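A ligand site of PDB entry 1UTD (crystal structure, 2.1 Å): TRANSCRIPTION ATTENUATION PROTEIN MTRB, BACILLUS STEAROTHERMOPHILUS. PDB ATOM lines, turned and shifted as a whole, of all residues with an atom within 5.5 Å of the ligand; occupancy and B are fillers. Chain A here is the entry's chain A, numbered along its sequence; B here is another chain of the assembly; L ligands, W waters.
The side-chain hydroxyl (OG1) of Thr 47 of chain B lies within hydrogen-bond range of the backbone NH (N) of Thr 50 of chain B (2.9 Å).
The side-chain hydroxyl (OG1) of Thr 47 of chain B lies close to the backbone NH (N) of His 49 of chain B, 3.1 Å away.
A ring nitrogen (NE2) of His 31 of chain B sits at hydrogen-bond distance from the side-chain hydroxyl (OG1) of Thr 50 of chain B (2.7 Å).
O of Ser 51 lies within hydrogen-bond range of N of Gln 45 of chain B, at 3.1 Å.
NH2 of Arg 24 is in hydrogen-bond range of OE1 of Gln 45 of chain B (2.7 Å).
The backbone NH of Ser 51 sits at hydrogen-bond distance from the backbone carbonyl oxygen of Leu 22.
The backbone carbonyl oxygen of Gly 21 of chain B lies within hydrogen-bond range of the backbone NH of His 31 of chain B, at 2.8 Å.
NE2 of His 49 of chain B lies close to N of Ala 26, 3.4 Å away.
The side-chain hydroxyl of Thr 47 of chain B is in hydrogen-bond range of an oxygen (O2) of the ligand, at 2.5 Å.
The backbone carbonyl oxygen of Thr 23 lies within hydrogen-bond range of a nitrogen (N1) of the ligand (2.8 Å).
OG1 of Thr 28 is in hydrogen-bond range of N1 of the ligand (2.8 Å).
N of Gly 25 sits at hydrogen-bond distance from O1 of the ligand.
The backbone carbonyl oxygen (O) of Gly 25 lies within hydrogen-bond range of a nitrogen (N1) of the ligand (2.9 Å).
O2 of the ligand lies within hydrogen-bond range of OG1 of Thr 50 of chain B, at 2.9 Å.
O of Gln 45 of chain B lies within hydrogen-bond range of N2 of the ligand (2.9 Å).
O1 of the ligand is in hydrogen-bond range of OG of Ser 51.
O of Asp 27 lies within hydrogen-bond range of N1 of the ligand (3.3 Å).
Water W1 lies within hydrogen-bond range of a ring nitrogen (ND1) of His 49 of chain B, an oxygen (O1) of the ligand, the backbone NH of Gly 25 and the side-chain hydroxyl of Thr 47 of chain B.
Merely in contact with the ligand: Arg 24 (3.5 Å), Gly 21 of chain B (3.5 Å), His 49 of chain B (3.9 Å), His 32 of chain B (3.9 Å), Ile 53 of chain B (3.9 Å) and Ala 44 of chain B (3.9 Å).
The nearest printed residue that does not touch the ligand is Ala 52 (4.1 Å).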
ATOM      1  N   LEU A  22     -15.419  18.160   6.063  1.00  0.00           N
ATOM      2  CA  LEU A  22     -15.875  19.566   6.045  1.00  0.00           C
ATOM      3  C   LEU A  22     -16.472  19.907   7.418  1.00  0.00           C
ATOM      4  O   LEU A  22     -17.244  19.099   7.965  1.00  0.00           O
ATOM      5  CB  LEU A  22     -16.903  19.813   4.925  1.00  0.00           C
ATOM      6  CG  LEU A  22     -16.421  19.905   3.461  1.00  0.00           C
ATOM      7  CD1 LEU A  22     -15.923  18.556   2.925  1.00  0.00           C
ATOM      8  CD2 LEU A  22     -17.464  20.420   2.536  1.00  0.00           C
ATOM      9  N   THR A  23     -16.118  21.072   7.966  1.00  0.00           N
ATOM     10  CA  THR A  23     -16.596  21.508   9.282  1.00  0.00           C
ATOM     11  C   THR A  23     -18.106  21.678   9.379  1.00  0.00           C
ATOM     12  O   THR A  23     -18.719  22.280   8.495  1.00  0.00           O
ATOM     13  CB  THR A  23     -15.985  22.863   9.683  1.00  0.00           C
ATOM     14  OG1 THR A  23     -16.256  23.826   8.654  1.00  0.00           O
ATOM     15  CG2 THR A  23     -14.443  22.787   9.807  1.00  0.00           C
ATOM     16  N   ARG A  24     -18.672  21.183  10.471  1.00  0.00           N
ATOM     17  CA  ARG A  24     -20.038  21.509  10.863  1.00  0.00           C
ATOM     18  C   ARG A  24     -20.123  22.951  11.354  1.00  0.00           C
ATOM     19  O   ARG A  24     -19.205  23.433  12.051  1.00  0.00           O
ATOM     20  CB  ARG A  24     -20.469  20.551  11.993  1.00  0.00           C
ATOM     21  CG  ARG A  24     -21.971  20.657  12.419  1.00  0.00           C
ATOM     22  CD  ARG A  24     -22.349  19.645  13.486  1.00  0.00           C
ATOM     23  NE  ARG A  24     -22.197  18.290  12.958  1.00  0.00           N
ATOM     24  CZ  ARG A  24     -23.112  17.692  12.200  1.00  0.00           C
ATOM     25  NH1 ARG A  24     -24.262  18.323  11.912  1.00  0.00           N
ATOM     26  NH2 ARG A  24     -22.908  16.445  11.755  1.00  0.00           N
ATOM     27  N   GLY A  25     -21.223  23.630  11.030  1.00  0.00           N
ATOM     28  CA  GLY A  25     -21.483  24.947  11.590  1.00  0.00           C
ATOM     29  C   GLY A  25     -21.735  26.018  10.533  1.00  0.00           C
ATOM     30  O   GLY A  25     -21.912  25.698   9.342  1.00  0.00           O
ATOM     31  N   ALA A  26     -21.764  27.283  10.952  1.00  0.00           N
ATOM     32  CA  ALA A  26     -21.941  28.430  10.048  1.00  0.00           C
ATOM     33  C   ALA A  26     -20.805  28.507   9.033  1.00  0.00           C
ATOM     34  O   ALA A  26     -21.030  28.913   7.899  1.00  0.00           O
ATOM     35  CB  ALA A  26     -22.060  29.764  10.847  1.00  0.00           C
ATOM     36  N   ASP A  27     -19.615  28.105   9.469  1.00  0.00           N
ATOM     37  CA  ASP A  27     -18.391  28.099   8.650  1.00  0.00           C
ATOM     38  C   ASP A  27     -18.111  26.751   7.990  1.00  0.00           C
ATOM     39  O   ASP A  27     -18.175  25.697   8.648  1.00  0.00           O
ATOM     40  CB  ASP A  27     -17.228  28.501   9.563  1.00  0.00           C
ATOM     41  CG  ASP A  27     -15.879  28.520   8.851  1.00  0.00           C
ATOM     42  OD1 ASP A  27     -15.535  29.578   8.244  1.00  0.00           O
ATOM     43  OD2 ASP A  27     -15.103  27.539   8.862  1.00  0.00           O
ATOM     44  N   THR A  28     -17.798  26.768   6.703  1.00  0.00           N
ATOM     45  CA  THR A  28     -17.472  25.553   5.953  1.00  0.00           C
ATOM     46  C   THR A  28     -16.051  25.596   5.362  1.00  0.00           C
ATOM     47  O   THR A  28     -15.741  26.407   4.492  1.00  0.00           O
ATOM     48  CB  THR A  28     -18.443  25.354   4.799  1.00  0.00           C
ATOM     49  OG1 THR A  28     -19.800  25.415   5.263  1.00  0.00           O
ATOM     50  CG2 THR A  28     -18.260  23.955   4.203  1.00  0.00           C
ATOM     51  N   SER A  51     -19.778  17.440   9.059  1.00  0.00           N
ATOM     52  CA  SER A  51     -21.156  17.307   8.560  1.00  0.00           C
ATOM     53  C   SER A  51     -21.183  17.084   7.064  1.00  0.00           C
ATOM     54  O   SER A  51     -22.269  17.019   6.445  1.00  0.00           O
ATOM     55  CB  SER A  51     -21.981  18.517   8.900  1.00  0.00           C
ATOM     56  OG  SER A  51     -21.354  19.663   8.351  1.00  0.00           O
ATOM     57  N   ALA A  52     -20.003  16.944   6.459  1.00  0.00           N
ATOM     58  CA  ALA A  52     -19.933  16.611   5.034  1.00  0.00           C
ATOM     59  C   ALA A  52     -18.563  16.016   4.757  1.00  0.00           C
ATOM     60  O   ALA A  52     -17.595  16.368   5.425  1.00  0.00           O
ATOM     61  CB  ALA A  52     -20.210  17.854   4.136  1.00  0.00           C
ATOM     62  N   VAL B  19     -22.494  22.246  -5.533  1.00  0.00           N
ATOM     63  CA  VAL B  19     -23.421  21.820  -4.499  1.00  0.00           C
ATOM     64  C   VAL B  19     -23.623  23.013  -3.557  1.00  0.00           C
ATOM     65  O   VAL B  19     -22.671  23.557  -2.988  1.00  0.00           O
ATOM     66  CB  VAL B  19     -22.910  20.546  -3.777  1.00  0.00           C
ATOM     67  CG1 VAL B  19     -23.967  20.029  -2.805  1.00  0.00           C
ATOM     68  CG2 VAL B  19     -22.614  19.443  -4.845  1.00  0.00           C
ATOM     69  N   ILE B  20     -24.881  23.461  -3.456  1.00  0.00           N
ATOM     70  CA  ILE B  20     -25.171  24.752  -2.864  1.00  0.00           C
ATOM     71  C   ILE B  20     -25.996  24.544  -1.600  1.00  0.00           C
ATOM     72  O   ILE B  20     -27.107  24.016  -1.668  1.00  0.00           O
ATOM     73  CB  ILE B  20     -25.944  25.652  -3.907  1.00  0.00           C
ATOM     74  CG1 ILE B  20     -25.072  25.963  -5.141  1.00  0.00           C
ATOM     75  CG2 ILE B  20     -26.470  26.943  -3.283  1.00  0.00           C
ATOM     76  CD1 ILE B  20     -25.940  26.487  -6.366  1.00  0.00           C
ATOM     77  N   GLY B  21     -25.475  25.011  -0.469  1.00  0.00           N
ATOM     78  CA  GLY B  21     -26.162  24.898   0.799  1.00  0.00           C
ATOM     79  C   GLY B  21     -26.951  26.138   1.113  1.00  0.00           C
ATOM     80  O   GLY B  21     -26.383  27.242   1.168  1.00  0.00           O
ATOM     81  N   HIS B  31     -25.297  29.747   1.757  1.00  0.00           N
ATOM     82  CA  HIS B  31     -24.159  30.137   2.655  1.00  0.00           C
ATOM     83  C   HIS B  31     -22.859  29.478   2.178  1.00  0.00           C
ATOM     84  O   HIS B  31     -21.757  29.881   2.594  1.00  0.00           O
ATOM     85  CB  HIS B  31     -24.413  29.811   4.151  1.00  0.00           C
ATOM     86  CG  HIS B  31     -24.578  28.346   4.412  1.00  0.00           C
ATOM     87  ND1 HIS B  31     -23.502  27.492   4.574  1.00  0.00           N
ATOM     88  CD2 HIS B  31     -25.677  27.559   4.440  1.00  0.00           C
ATOM     89  CE1 HIS B  31     -23.940  26.250   4.727  1.00  0.00           C
ATOM     90  NE2 HIS B  31     -25.257  26.261   4.650  1.00  0.00           N
ATOM     91  N   HIS B  32     -22.976  28.481   1.316  1.00  0.00           N
ATOM     92  CA  HIS B  32     -21.797  27.782   0.868  1.00  0.00           C
ATOM     93  C   HIS B  32     -22.037  27.119  -0.467  1.00  0.00           C
ATOM     94  O   HIS B  32     -23.122  26.618  -0.720  1.00  0.00           O
ATOM     95  CB  HIS B  32     -21.327  26.703   1.868  1.00  0.00           C
ATOM     96  CG  HIS B  32     -20.032  26.047   1.472  1.00  0.00           C
ATOM     97  ND1 HIS B  32     -18.808  26.674   1.610  1.00  0.00           N
ATOM     98  CD2 HIS B  32     -19.769  24.844   0.892  1.00  0.00           C
ATOM     99  CE1 HIS B  32     -17.851  25.891   1.126  1.00  0.00           C
ATOM    100  NE2 HIS B  32     -18.410  24.760   0.711  1.00  0.00           N
ATOM    101  N   SER B  33     -21.012  27.106  -1.294  1.00  0.00           N
ATOM    102  CA  SER B  33     -21.094  26.454  -2.586  1.00  0.00           C
ATOM    103  C   SER B  33     -19.855  25.584  -2.677  1.00  0.00           C
ATOM    104  O   SER B  33     -18.758  26.095  -2.552  1.00  0.00           O
ATOM    105  CB  SER B  33     -21.088  27.561  -3.663  1.00  0.00           C
ATOM    106  OG  SER B  33     -20.272  27.205  -4.758  1.00  0.00           O
ATOM    107  N   GLU B  34     -20.033  24.269  -2.782  1.00  0.00           N
ATOM    108  CA  GLU B  34     -18.885  23.377  -2.868  1.00  0.00           C
ATOM    109  C   GLU B  34     -18.793  22.904  -4.320  1.00  0.00           C
ATOM    110  O   GLU B  34     -19.713  22.255  -4.812  1.00  0.00           O
ATOM    111  CB  GLU B  34     -19.044  22.211  -1.877  1.00  0.00           C
ATOM    112  CG  GLU B  34     -17.840  21.272  -1.770  1.00  0.00           C
ATOM    113  CD  GLU B  34     -16.601  21.963  -1.229  1.00  0.00           C
ATOM    114  OE1 GLU B  34     -16.730  22.895  -0.396  1.00  0.00           O
ATOM    115  OE2 GLU B  34     -15.478  21.587  -1.633  1.00  0.00           O
ATOM    116  N   ALA B  44     -23.195  14.726   2.030  1.00  0.00           N
ATOM    117  CA  ALA B  44     -23.489  15.966   2.730  1.00  0.00           C
ATOM    118  C   ALA B  44     -24.782  15.847   3.541  1.00  0.00           C
ATOM    119  O   ALA B  44     -25.806  15.464   2.978  1.00  0.00           O
ATOM    120  CB  ALA B  44     -23.615  17.122   1.681  1.00  0.00           C
ATOM    121  N   GLN B  45     -24.730  16.197   4.815  1.00  0.00           N
ATOM    122  CA  GLN B  45     -25.882  16.119   5.705  1.00  0.00           C
ATOM    123  C   GLN B  45     -26.759  17.372   5.645  1.00  0.00           C
ATOM    124  O   GLN B  45     -26.288  18.454   5.269  1.00  0.00           O
ATOM    125  CB  GLN B  45     -25.437  15.958   7.162  1.00  0.00           C
ATOM    126  CG  GLN B  45     -24.956  14.566   7.571  1.00  0.00           C
ATOM    127  CD  GLN B  45     -24.675  14.474   9.049  1.00  0.00           C
ATOM    128  OE1 GLN B  45     -23.930  15.297   9.593  1.00  0.00           O
ATOM    129  NE2 GLN B  45     -25.261  13.465   9.730  1.00  0.00           N
ATOM    130  N   PHE B  46     -28.013  17.236   6.077  1.00  0.00           N
ATOM    131  CA  PHE B  46     -28.761  18.428   6.489  1.00  0.00           C
ATOM    132  C   PHE B  46     -28.331  18.696   7.913  1.00  0.00           C
ATOM    133  O   PHE B  46     -28.021  17.746   8.631  1.00  0.00           O
ATOM    134  CB  PHE B  46     -30.285  18.190   6.426  1.00  0.00           C
ATOM    135  CG  PHE B  46     -30.804  18.136   5.024  1.00  0.00           C
ATOM    136  CD1 PHE B  46     -30.832  19.274   4.234  1.00  0.00           C
ATOM    137  CD2 PHE B  46     -31.280  16.946   4.493  1.00  0.00           C
ATOM    138  CE1 PHE B  46     -31.320  19.223   2.913  1.00  0.00           C
ATOM    139  CE2 PHE B  46     -31.768  16.888   3.179  1.00  0.00           C
ATOM    140  CZ  PHE B  46     -31.779  18.011   2.386  1.00  0.00           C
ATOM    141  N   THR B  47     -28.255  19.978   8.290  1.00  0.00           N
ATOM    142  CA  THR B  47     -27.607  20.375   9.541  1.00  0.00           C
ATOM    143  C   THR B  47     -28.366  21.534  10.195  1.00  0.00           C
ATOM    144  O   THR B  47     -29.309  22.070   9.590  1.00  0.00           O
ATOM    145  CB  THR B  47     -26.149  20.863   9.265  1.00  0.00           C
ATOM    146  OG1 THR B  47     -26.182  22.011   8.408  1.00  0.00           O
ATOM    147  CG2 THR B  47     -25.354  19.849   8.442  1.00  0.00           C
ATOM    148  N   HIS B  49     -27.281  24.361  10.063  1.00  0.00           N
ATOM    149  CA  HIS B  49     -27.078  25.532   9.155  1.00  0.00           C
ATOM    150  C   HIS B  49     -27.619  25.365   7.711  1.00  0.00           C
ATOM    151  O   HIS B  49     -27.860  26.348   7.032  1.00  0.00           O
ATOM    152  CB  HIS B  49     -25.616  26.019   9.173  1.00  0.00           C
ATOM    153  CG  HIS B  49     -25.237  26.584  10.485  1.00  0.00           C
ATOM    154  ND1 HIS B  49     -24.823  25.798  11.554  1.00  0.00           N
ATOM    155  CD2 HIS B  49     -25.305  27.858  10.962  1.00  0.00           C
ATOM    156  CE1 HIS B  49     -24.619  26.567  12.611  1.00  0.00           C
ATOM    157  NE2 HIS B  49     -24.891  27.825  12.276  1.00  0.00           N
ATOM    158  N   THR B  50     -27.862  24.130   7.298  1.00  0.00           N
ATOM    159  CA  THR B  50     -28.333  23.811   5.953  1.00  0.00           C
ATOM    160  C   THR B  50     -29.628  22.977   5.988  1.00  0.00           C
ATOM    161  O   THR B  50     -29.614  21.844   6.442  1.00  0.00           O
ATOM    162  CB  THR B  50     -27.248  23.013   5.262  1.00  0.00           C
ATOM    163  OG1 THR B  50     -26.033  23.797   5.276  1.00  0.00           O
ATOM    164  CG2 THR B  50     -27.580  22.788   3.781  1.00  0.00           C
ATOM    165  N   ILE B  53     -30.542  21.772  -0.041  1.00  0.00           N
ATOM    166  CA  ILE B  53     -29.358  21.630  -0.898  1.00  0.00           C
ATOM    167  C   ILE B  53     -29.767  21.722  -2.391  1.00  0.00           C
ATOM    168  O   ILE B  53     -30.726  21.028  -2.827  1.00  0.00           O
ATOM    169  CB  ILE B  53     -28.661  20.277  -0.615  1.00  0.00           C
ATOM    170  CG1 ILE B  53     -28.211  20.160   0.864  1.00  0.00           C
ATOM    171  CG2 ILE B  53     -27.491  20.040  -1.584  1.00  0.00           C
ATOM    172  CD1 ILE B  53     -27.736  18.747   1.279  1.00  0.00           C
HETATM  173  N1  LIG L   1     -20.719  23.906   7.450  1.00  0.00           N
HETATM  174  C1  LIG L   1     -21.851  23.300   6.698  1.00  0.00           C
HETATM  175  C2  LIG L   1     -22.960  22.819   7.653  1.00  0.00           C
HETATM  176  O1  LIG L   1     -22.666  22.261   8.745  1.00  0.00           O
HETATM  177  C3  LIG L   1     -21.358  22.137   5.808  1.00  0.00           C
HETATM  178  C4  LIG L   1     -22.453  21.468   4.966  1.00  0.00           C
HETATM  179  C5  LIG L   1     -23.226  20.361   5.312  1.00  0.00           C
HETATM  180  C6  LIG L   1     -22.884  21.854   3.653  1.00  0.00           C
HETATM  181  N2  LIG L   1     -24.095  20.049   4.288  1.00  0.00           N
HETATM  182  C7  LIG L   1     -23.910  20.951   3.262  1.00  0.00           C
HETATM  183  C8  LIG L   1     -22.528  22.876   2.769  1.00  0.00           C
HETATM  184  C9  LIG L   1     -24.560  21.038   2.028  1.00  0.00           C
HETATM  185  C10 LIG L   1     -23.142  22.948   1.548  1.00  0.00           C
HETATM  186  C11 LIG L   1     -24.165  22.043   1.188  1.00  0.00           C
HETATM  187  O2  LIG L   1     -24.133  23.007   7.288  1.00  0.00           O
HETATM  188  O   HOH W   1     -24.370  23.118  11.001  1.00  0.00           O
